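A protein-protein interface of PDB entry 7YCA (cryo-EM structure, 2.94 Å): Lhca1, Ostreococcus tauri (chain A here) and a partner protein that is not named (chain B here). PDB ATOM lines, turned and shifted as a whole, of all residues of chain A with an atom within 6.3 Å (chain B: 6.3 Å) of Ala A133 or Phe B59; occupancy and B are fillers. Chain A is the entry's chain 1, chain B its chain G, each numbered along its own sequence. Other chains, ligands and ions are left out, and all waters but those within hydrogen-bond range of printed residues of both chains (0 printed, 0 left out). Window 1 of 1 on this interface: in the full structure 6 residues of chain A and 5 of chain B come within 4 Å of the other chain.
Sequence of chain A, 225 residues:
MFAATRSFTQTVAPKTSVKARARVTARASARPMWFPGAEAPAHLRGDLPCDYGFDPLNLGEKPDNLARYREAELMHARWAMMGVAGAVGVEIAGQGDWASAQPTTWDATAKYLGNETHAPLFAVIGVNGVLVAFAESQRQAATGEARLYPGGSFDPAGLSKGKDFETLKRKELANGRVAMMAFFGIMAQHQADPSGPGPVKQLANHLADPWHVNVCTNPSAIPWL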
ATOM      1  N   ASN A 128       5.457  20.802   7.549  1.00  0.00           N
ATOM      2  CA  ASN A 128       4.876  21.833   6.693  1.00  0.00           C
ATOM      3  C   ASN A 128       3.411  22.055   7.042  1.00  0.00           C
ATOM      4  O   ASN A 128       2.936  23.198   7.080  1.00  0.00           O
ATOM      5  CB  ASN A 128       5.013  21.453   5.214  1.00  0.00           C
ATOM      6  CG  ASN A 128       6.416  20.995   4.845  1.00  0.00           C
ATOM      7  OD1 ASN A 128       6.821  19.882   5.176  1.00  0.00           O
ATOM      8  ND2 ASN A 128       7.160  21.850   4.153  1.00  0.00           N
ATOM      9  N   GLY A 129       2.689  20.966   7.319  1.00  0.00           N
ATOM     10  CA  GLY A 129       1.255  21.062   7.532  1.00  0.00           C
ATOM     11  C   GLY A 129       0.883  21.889   8.748  1.00  0.00           C
ATOM     12  O   GLY A 129      -0.020  22.722   8.679  1.00  0.00           O
ATOM     13  N   VAL A 130       1.574  21.677   9.873  1.00  0.00           N
ATOM     14  CA  VAL A 130       1.224  22.408  11.098  1.00  0.00           C
ATOM     15  C   VAL A 130       1.484  23.904  10.930  1.00  0.00           C
ATOM     16  O   VAL A 130       0.644  24.738  11.296  1.00  0.00           O
ATOM     17  CB  VAL A 130       1.958  21.858  12.345  1.00  0.00           C
ATOM     18  CG1 VAL A 130       1.237  20.626  12.898  1.00  0.00           C
ATOM     19  CG2 VAL A 130       3.478  21.611  12.154  1.00  0.00           C
ATOM     20  N   LEU A 131       2.645  24.266  10.379  1.00  0.00           N
ATOM     21  CA  LEU A 131       2.975  25.680  10.228  1.00  0.00           C
ATOM     22  C   LEU A 131       2.038  26.365   9.244  1.00  0.00           C
ATOM     23  O   LEU A 131       1.564  27.481   9.503  1.00  0.00           O
ATOM     24  CB  LEU A 131       4.429  25.839   9.782  1.00  0.00           C
ATOM     25  CG  LEU A 131       5.507  25.167  10.644  1.00  0.00           C
ATOM     26  CD1 LEU A 131       6.894  25.489  10.096  1.00  0.00           C
ATOM     27  CD2 LEU A 131       5.420  25.526  12.126  1.00  0.00           C
ATOM     28  N   VAL A 132       1.744  25.713   8.116  1.00  0.00           N
ATOM     29  CA  VAL A 132       0.847  26.329   7.147  1.00  0.00           C
ATOM     30  C   VAL A 132      -0.568  26.405   7.709  1.00  0.00           C
ATOM     31  O   VAL A 132      -1.298  27.360   7.434  1.00  0.00           O
ATOM     32  CB  VAL A 132       0.898  25.578   5.801  1.00  0.00           C
ATOM     33  CG1 VAL A 132      -0.085  26.181   4.804  1.00  0.00           C
ATOM     34  CG2 VAL A 132       2.298  25.654   5.193  1.00  0.00           C
ATOM     35  N   ALA A 133      -0.984  25.403   8.491  1.00  0.00           N
ATOM     36  CA  ALA A 133      -2.305  25.448   9.105  1.00  0.00           C
ATOM     37  C   ALA A 133      -2.419  26.611  10.077  1.00  0.00           C
ATOM     38  O   ALA A 133      -3.437  27.312  10.093  1.00  0.00           O
ATOM     39  CB  ALA A 133      -2.603  24.130   9.818  1.00  0.00           C
ATOM     40  N   PHE A 134      -1.378  26.843  10.881  1.00  0.00           N
ATOM     41  CA  PHE A 134      -1.400  27.983  11.791  1.00  0.00           C
ATOM     42  C   PHE A 134      -1.458  29.295  11.005  1.00  0.00           C
ATOM     43  O   PHE A 134      -2.276  30.174  11.308  1.00  0.00           O
ATOM     44  CB  PHE A 134      -0.168  27.935  12.717  1.00  0.00           C
ATOM     45  CG  PHE A 134      -0.270  28.782  13.999  1.00  0.00           C
ATOM     46  CD1 PHE A 134      -1.271  29.717  14.203  1.00  0.00           C
ATOM     47  CD2 PHE A 134       0.675  28.635  15.002  1.00  0.00           C
ATOM     48  CE1 PHE A 134      -1.332  30.448  15.318  1.00  0.00           C
ATOM     49  CE2 PHE A 134       0.599  29.399  16.158  1.00  0.00           C
ATOM     50  CZ  PHE A 134      -0.415  30.308  16.303  1.00  0.00           C
ATOM     51  N   ALA A 135      -0.602  29.438   9.989  1.00  0.00           N
ATOM     52  CA  ALA A 135      -0.568  30.685   9.227  1.00  0.00           C
ATOM     53  C   ALA A 135      -1.894  30.938   8.519  1.00  0.00           C
ATOM     54  O   ALA A 135      -2.398  32.068   8.502  1.00  0.00           O
ATOM     55  CB  ALA A 135       0.576  30.645   8.216  1.00  0.00           C
ATOM     56  N   GLU A 136      -2.491  29.886   7.963  1.00  0.00           N
ATOM     57  CA  GLU A 136      -3.742  30.029   7.231  1.00  0.00           C
ATOM     58  C   GLU A 136      -4.910  30.308   8.164  1.00  0.00           C
ATOM     59  O   GLU A 136      -5.806  31.087   7.820  1.00  0.00           O
ATOM     60  CB  GLU A 136      -3.990  28.768   6.411  1.00  0.00           C
ATOM     61  CG  GLU A 136      -3.179  28.760   5.120  1.00  0.00           C
ATOM     62  CD  GLU A 136      -3.917  29.345   3.933  1.00  0.00           C
ATOM     63  OE1 GLU A 136      -5.011  29.917   4.115  1.00  0.00           O
ATOM     64  OE2 GLU A 136      -3.394  29.245   2.805  1.00  0.00           O
ATOM     65  N   SER A 137      -4.925  29.684   9.345  1.00  0.00           N
ATOM     66  CA  SER A 137      -5.954  30.006  10.326  1.00  0.00           C
ATOM     67  C   SER A 137      -5.843  31.457  10.767  1.00  0.00           C
ATOM     68  O   SER A 137      -6.859  32.147  10.922  1.00  0.00           O
ATOM     69  CB  SER A 137      -5.846  29.069  11.529  1.00  0.00           C
ATOM     70  OG  SER A 137      -4.622  29.256  12.218  1.00  0.00           O
ATOM     71  N   GLN A 138      -4.613  31.942  10.964  1.00  0.00           N
ATOM     72  CA  GLN A 138      -4.438  33.336  11.355  1.00  0.00           C
ATOM     73  C   GLN A 138      -4.881  34.283  10.248  1.00  0.00           C
ATOM     74  O   GLN A 138      -5.482  35.328  10.524  1.00  0.00           O
ATOM     75  CB  GLN A 138      -2.975  33.610  11.736  1.00  0.00           C
ATOM     76  CG  GLN A 138      -2.550  33.254  13.181  1.00  0.00           C
ATOM     77  CD  GLN A 138      -3.445  33.884  14.259  1.00  0.00           C
ATOM     78  OE1 GLN A 138      -4.163  34.841  13.991  1.00  0.00           O
ATOM     79  NE2 GLN A 138      -3.413  33.338  15.463  1.00  0.00           N
ATOM     80  N   LEU B  54      -2.807  21.001  18.663  1.00  0.00           N
ATOM     81  CA  LEU B  54      -3.355  21.658  17.489  1.00  0.00           C
ATOM     82  C   LEU B  54      -4.829  21.939  17.695  1.00  0.00           C
ATOM     83  O   LEU B  54      -5.310  23.035  17.400  1.00  0.00           O
ATOM     84  CB  LEU B  54      -3.155  20.765  16.268  1.00  0.00           C
ATOM     85  CG  LEU B  54      -3.518  21.309  14.889  1.00  0.00           C
ATOM     86  CD1 LEU B  54      -2.602  22.464  14.522  1.00  0.00           C
ATOM     87  CD2 LEU B  54      -3.394  20.194  13.861  1.00  0.00           C
ATOM     88  N   GLY B  55      -5.552  20.949  18.208  1.00  0.00           N
ATOM     89  CA  GLY B  55      -6.968  21.138  18.468  1.00  0.00           C
ATOM     90  C   GLY B  55      -7.205  22.157  19.558  1.00  0.00           C
ATOM     91  O   GLY B  55      -8.170  22.921  19.499  1.00  0.00           O
ATOM     92  N   ARG B  56      -6.328  22.179  20.554  1.00  0.00           N
ATOM     93  CA  ARG B  56      -6.481  23.101  21.676  1.00  0.00           C
ATOM     94  C   ARG B  56      -6.278  24.571  21.306  1.00  0.00           C
ATOM     95  O   ARG B  56      -6.894  25.453  21.906  1.00  0.00           O
ATOM     96  CB  ARG B  56      -5.514  22.709  22.802  1.00  0.00           C
ATOM     97  CG  ARG B  56      -5.484  23.680  23.968  1.00  0.00           C
ATOM     98  CD  ARG B  56      -6.839  23.793  24.643  1.00  0.00           C
ATOM     99  NE  ARG B  56      -6.961  25.034  25.403  1.00  0.00           N
ATOM    100  CZ  ARG B  56      -6.616  25.170  26.679  1.00  0.00           C
ATOM    101  NH1 ARG B  56      -6.121  24.141  27.345  1.00  0.00           N
ATOM    102  NH2 ARG B  56      -6.763  26.337  27.289  1.00  0.00           N
ATOM    103  N   PHE B  57      -5.424  24.853  20.327  1.00  0.00           N
ATOM    104  CA  PHE B  57      -5.136  26.270  20.022  1.00  0.00           C
ATOM    105  C   PHE B  57      -5.399  26.767  18.597  1.00  0.00           C
ATOM    106  O   PHE B  57      -5.896  27.896  18.403  1.00  0.00           O
ATOM    107  CB  PHE B  57      -3.676  26.569  20.388  1.00  0.00           C
ATOM    108  CG  PHE B  57      -3.278  26.068  21.747  1.00  0.00           C
ATOM    109  CD1 PHE B  57      -3.672  26.740  22.892  1.00  0.00           C
ATOM    110  CD2 PHE B  57      -2.506  24.927  21.881  1.00  0.00           C
ATOM    111  CE1 PHE B  57      -3.307  26.281  24.144  1.00  0.00           C
ATOM    112  CE2 PHE B  57      -2.138  24.460  23.128  1.00  0.00           C
ATOM    113  CZ  PHE B  57      -2.538  25.140  24.262  1.00  0.00           C
ATOM    114  N   VAL B  58      -5.078  25.952  17.600  1.00  0.00           N
ATOM    115  CA  VAL B  58      -5.201  26.402  16.212  1.00  0.00           C
ATOM    116  C   VAL B  58      -6.662  26.368  15.780  1.00  0.00           C
ATOM    117  O   VAL B  58      -7.247  27.429  15.529  1.00  0.00           O
ATOM    118  CB  VAL B  58      -4.283  25.572  15.290  1.00  0.00           C
ATOM    119  CG1 VAL B  58      -4.248  26.122  13.867  1.00  0.00           C
ATOM    120  CG2 VAL B  58      -2.852  25.597  15.836  1.00  0.00           C
ATOM    121  N   PHE B  59      -7.275  25.184  15.713  1.00  0.00           N
ATOM    122  CA  PHE B  59      -8.645  25.079  15.218  1.00  0.00           C
ATOM    123  C   PHE B  59      -9.677  25.035  16.333  1.00  0.00           C
ATOM    124  O   PHE B  59     -10.844  24.779  16.047  1.00  0.00           O
ATOM    125  CB  PHE B  59      -8.860  23.850  14.329  1.00  0.00           C
ATOM    126  CG  PHE B  59      -7.663  23.416  13.529  1.00  0.00           C
ATOM    127  CD1 PHE B  59      -6.920  24.263  12.740  1.00  0.00           C
ATOM    128  CD2 PHE B  59      -7.340  22.107  13.536  1.00  0.00           C
ATOM    129  CE1 PHE B  59      -5.836  23.771  12.025  1.00  0.00           C
ATOM    130  CE2 PHE B  59      -6.320  21.596  12.827  1.00  0.00           C
ATOM    131  CZ  PHE B  59      -5.541  22.424  12.072  1.00  0.00           C
ATOM    132  N   LEU B  60      -9.290  25.248  17.593  1.00  0.00           N
ATOM    133  CA  LEU B  60     -10.313  25.359  18.630  1.00  0.00           C
ATOM    134  C   LEU B  60     -11.232  26.556  18.440  1.00  0.00           C
ATOM    135  O   LEU B  60     -12.455  26.378  18.579  1.00  0.00           O
ATOM    136  CB  LEU B  60      -9.697  25.409  20.033  1.00  0.00           C
ATOM    137  CG  LEU B  60     -10.621  25.265  21.265  1.00  0.00           C
ATOM    138  CD1 LEU B  60     -11.735  24.237  21.096  1.00  0.00           C
ATOM    139  CD2 LEU B  60      -9.831  24.873  22.471  1.00  0.00           C
ATOM    140  N   PRO B  61     -10.744  27.788  18.197  1.00  0.00           N
ATOM    141  CA  PRO B  61     -11.703  28.883  17.963  1.00  0.00           C
ATOM    142  C   PRO B  61     -12.587  28.647  16.757  1.00  0.00           C
ATOM    143  O   PRO B  61     -13.785  28.947  16.806  1.00  0.00           O
ATOM    144  CB  PRO B  61     -10.798  30.109  17.773  1.00  0.00           C
ATOM    145  CG  PRO B  61      -9.497  29.556  17.380  1.00  0.00           C
ATOM    146  CD  PRO B  61      -9.364  28.318  18.189  1.00  0.00           C
ATOM    147  N   TYR B  62     -12.037  28.061  15.693  1.00  0.00           N
ATOM    148  CA  TYR B  62     -12.850  27.762  14.523  1.00  0.00           C
ATOM    149  C   TYR B  62     -13.890  26.698  14.834  1.00  0.00           C
ATOM    150  O   TYR B  62     -15.051  26.831  14.441  1.00  0.00           O
ATOM    151  CB  TYR B  62     -11.964  27.316  13.363  1.00  0.00           C
ATOM    152  CG  TYR B  62     -12.738  27.035  12.098  1.00  0.00           C
ATOM    153  CD1 TYR B  62     -13.269  28.066  11.343  1.00  0.00           C
ATOM    154  CD2 TYR B  62     -12.942  25.740  11.660  1.00  0.00           C
ATOM    155  CE1 TYR B  62     -13.983  27.808  10.191  1.00  0.00           C
ATOM    156  CE2 TYR B  62     -13.642  25.481  10.496  1.00  0.00           C
ATOM    157  CZ  TYR B  62     -14.165  26.515   9.772  1.00  0.00           C
ATOM    158  OH  TYR B  62     -14.870  26.245   8.622  1.00  0.00           O
ATOM    159  N   GLN B  63     -13.500  25.642  15.552  1.00  0.00           N
ATOM    160  CA  GLN B  63     -14.445  24.582  15.880  1.00  0.00           C
ATOM    161  C   GLN B  63     -15.560  25.099  16.778  1.00  0.00           C
ATOM    162  O   GLN B  63     -16.737  24.792  16.560  1.00  0.00           O
ATOM    163  CB  GLN B  63     -13.709  23.412  16.545  1.00  0.00           C
ATOM    164  CG  GLN B  63     -14.569  22.192  16.800  1.00  0.00           C
ATOM    165  CD  GLN B  63     -13.806  20.987  17.299  1.00  0.00           C
ATOM    166  OE1 GLN B  63     -12.578  21.004  17.386  1.00  0.00           O
ATOM    167  NE2 GLN B  63     -14.533  19.917  17.614  1.00  0.00           N
ATOM    168  N   ARG B  64     -15.213  25.910  17.780  1.00  0.00           N
ATOM    169  CA  ARG B  64     -16.232  26.455  18.671  1.00  0.00           C
ATOM    170  C   ARG B  64     -17.133  27.445  17.941  1.00  0.00           C
ATOM    171  O   ARG B  64     -18.341  27.510  18.199  1.00  0.00           O
ATOM    172  CB  ARG B  64     -15.589  27.119  19.880  1.00  0.00           C
ATOM    173  CG  ARG B  64     -14.851  26.144  20.762  1.00  0.00           C
ATOM    174  CD  ARG B  64     -14.112  26.835  21.888  1.00  0.00           C
ATOM    175  NE  ARG B  64     -14.955  26.968  23.071  1.00  0.00           N
ATOM    176  CZ  ARG B  64     -15.095  26.061  24.035  1.00  0.00           C
ATOM    177  NH1 ARG B  64     -14.434  24.911  24.022  1.00  0.00           N
ATOM    178  NH2 ARG B  64     -15.924  26.315  25.040  1.00  0.00           N
ATOM    179  N   TRP B 111      -9.458  14.727  19.368  1.00  0.00           N
ATOM    180  CA  TRP B 111      -8.124  15.074  18.889  1.00  0.00           C
ATOM    181  C   TRP B 111      -7.120  13.957  19.134  1.00  0.00           C
ATOM    182  O   TRP B 111      -6.189  13.784  18.343  1.00  0.00           O
ATOM    183  CB  TRP B 111      -7.670  16.378  19.539  1.00  0.00           C
ATOM    184  CG  TRP B 111      -8.409  17.508  18.979  1.00  0.00           C
ATOM    185  CD1 TRP B 111      -9.403  18.225  19.572  1.00  0.00           C
ATOM    186  CD2 TRP B 111      -8.266  18.027  17.671  1.00  0.00           C
ATOM    187  NE1 TRP B 111      -9.881  19.172  18.714  1.00  0.00           N
ATOM    188  CE2 TRP B 111      -9.183  19.083  17.542  1.00  0.00           C
ATOM    189  CE3 TRP B 111      -7.433  17.717  16.597  1.00  0.00           C
ATOM    190  CZ2 TRP B 111      -9.312  19.794  16.385  1.00  0.00           C
ATOM    191  CZ3 TRP B 111      -7.552  18.438  15.463  1.00  0.00           C
ATOM    192  CH2 TRP B 111      -8.485  19.453  15.362  1.00  0.00           C
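Ala A133 touches just one residue of chain B: Phe B59 (3.9 Å). Phe B59 touches just one residue of chain A: Ala A133. Printed residues of chain B within 4 Å of Phe A134: Val B58. Of the printed residues of chain A, Val B58 touches Phe A134 and Ser A137. Of the printed residues of chain B, Ser A137 touches Val B58 (3.6 Å). Val A130 touches none of the printed residues of chain B. Ala A135 touches none of the printed residues of chain B. The nearest residue of chain B that does not touch Ala A133 is Val B58 (4.04 Å). The nearest printed residue of chain B that does not touch Phe A134 is Phe B59 (5.5 Å).
The backbone carbonyl oxygen (O) of Ala A133 sits at hydrogen-bond distance from the side-chain hydroxyl (OG) of Ser A137, 3.1 Å away. The side-chain hydroxyl (OG) of Ser A137 sits at hydrogen-bond distance from the backbone carbonyl oxygen (O) of Phe A134 (2.7 Å). The backbone carbonyl oxygen of Leu B54 lies within hydrogen-bond range of the backbone NH of Phe B59, 3.4 Å away.
Hydrophobic or aromatic side chains of chain A that line the printed part of chain B: Ala A133.
Among the printed residues, merely in contact across the chains: Ser A137 with Val B58 (3.6 Å), Ala A133 with Phe B59 (3.9 Å) and Phe A134 with Val B58 (3.99 Å).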
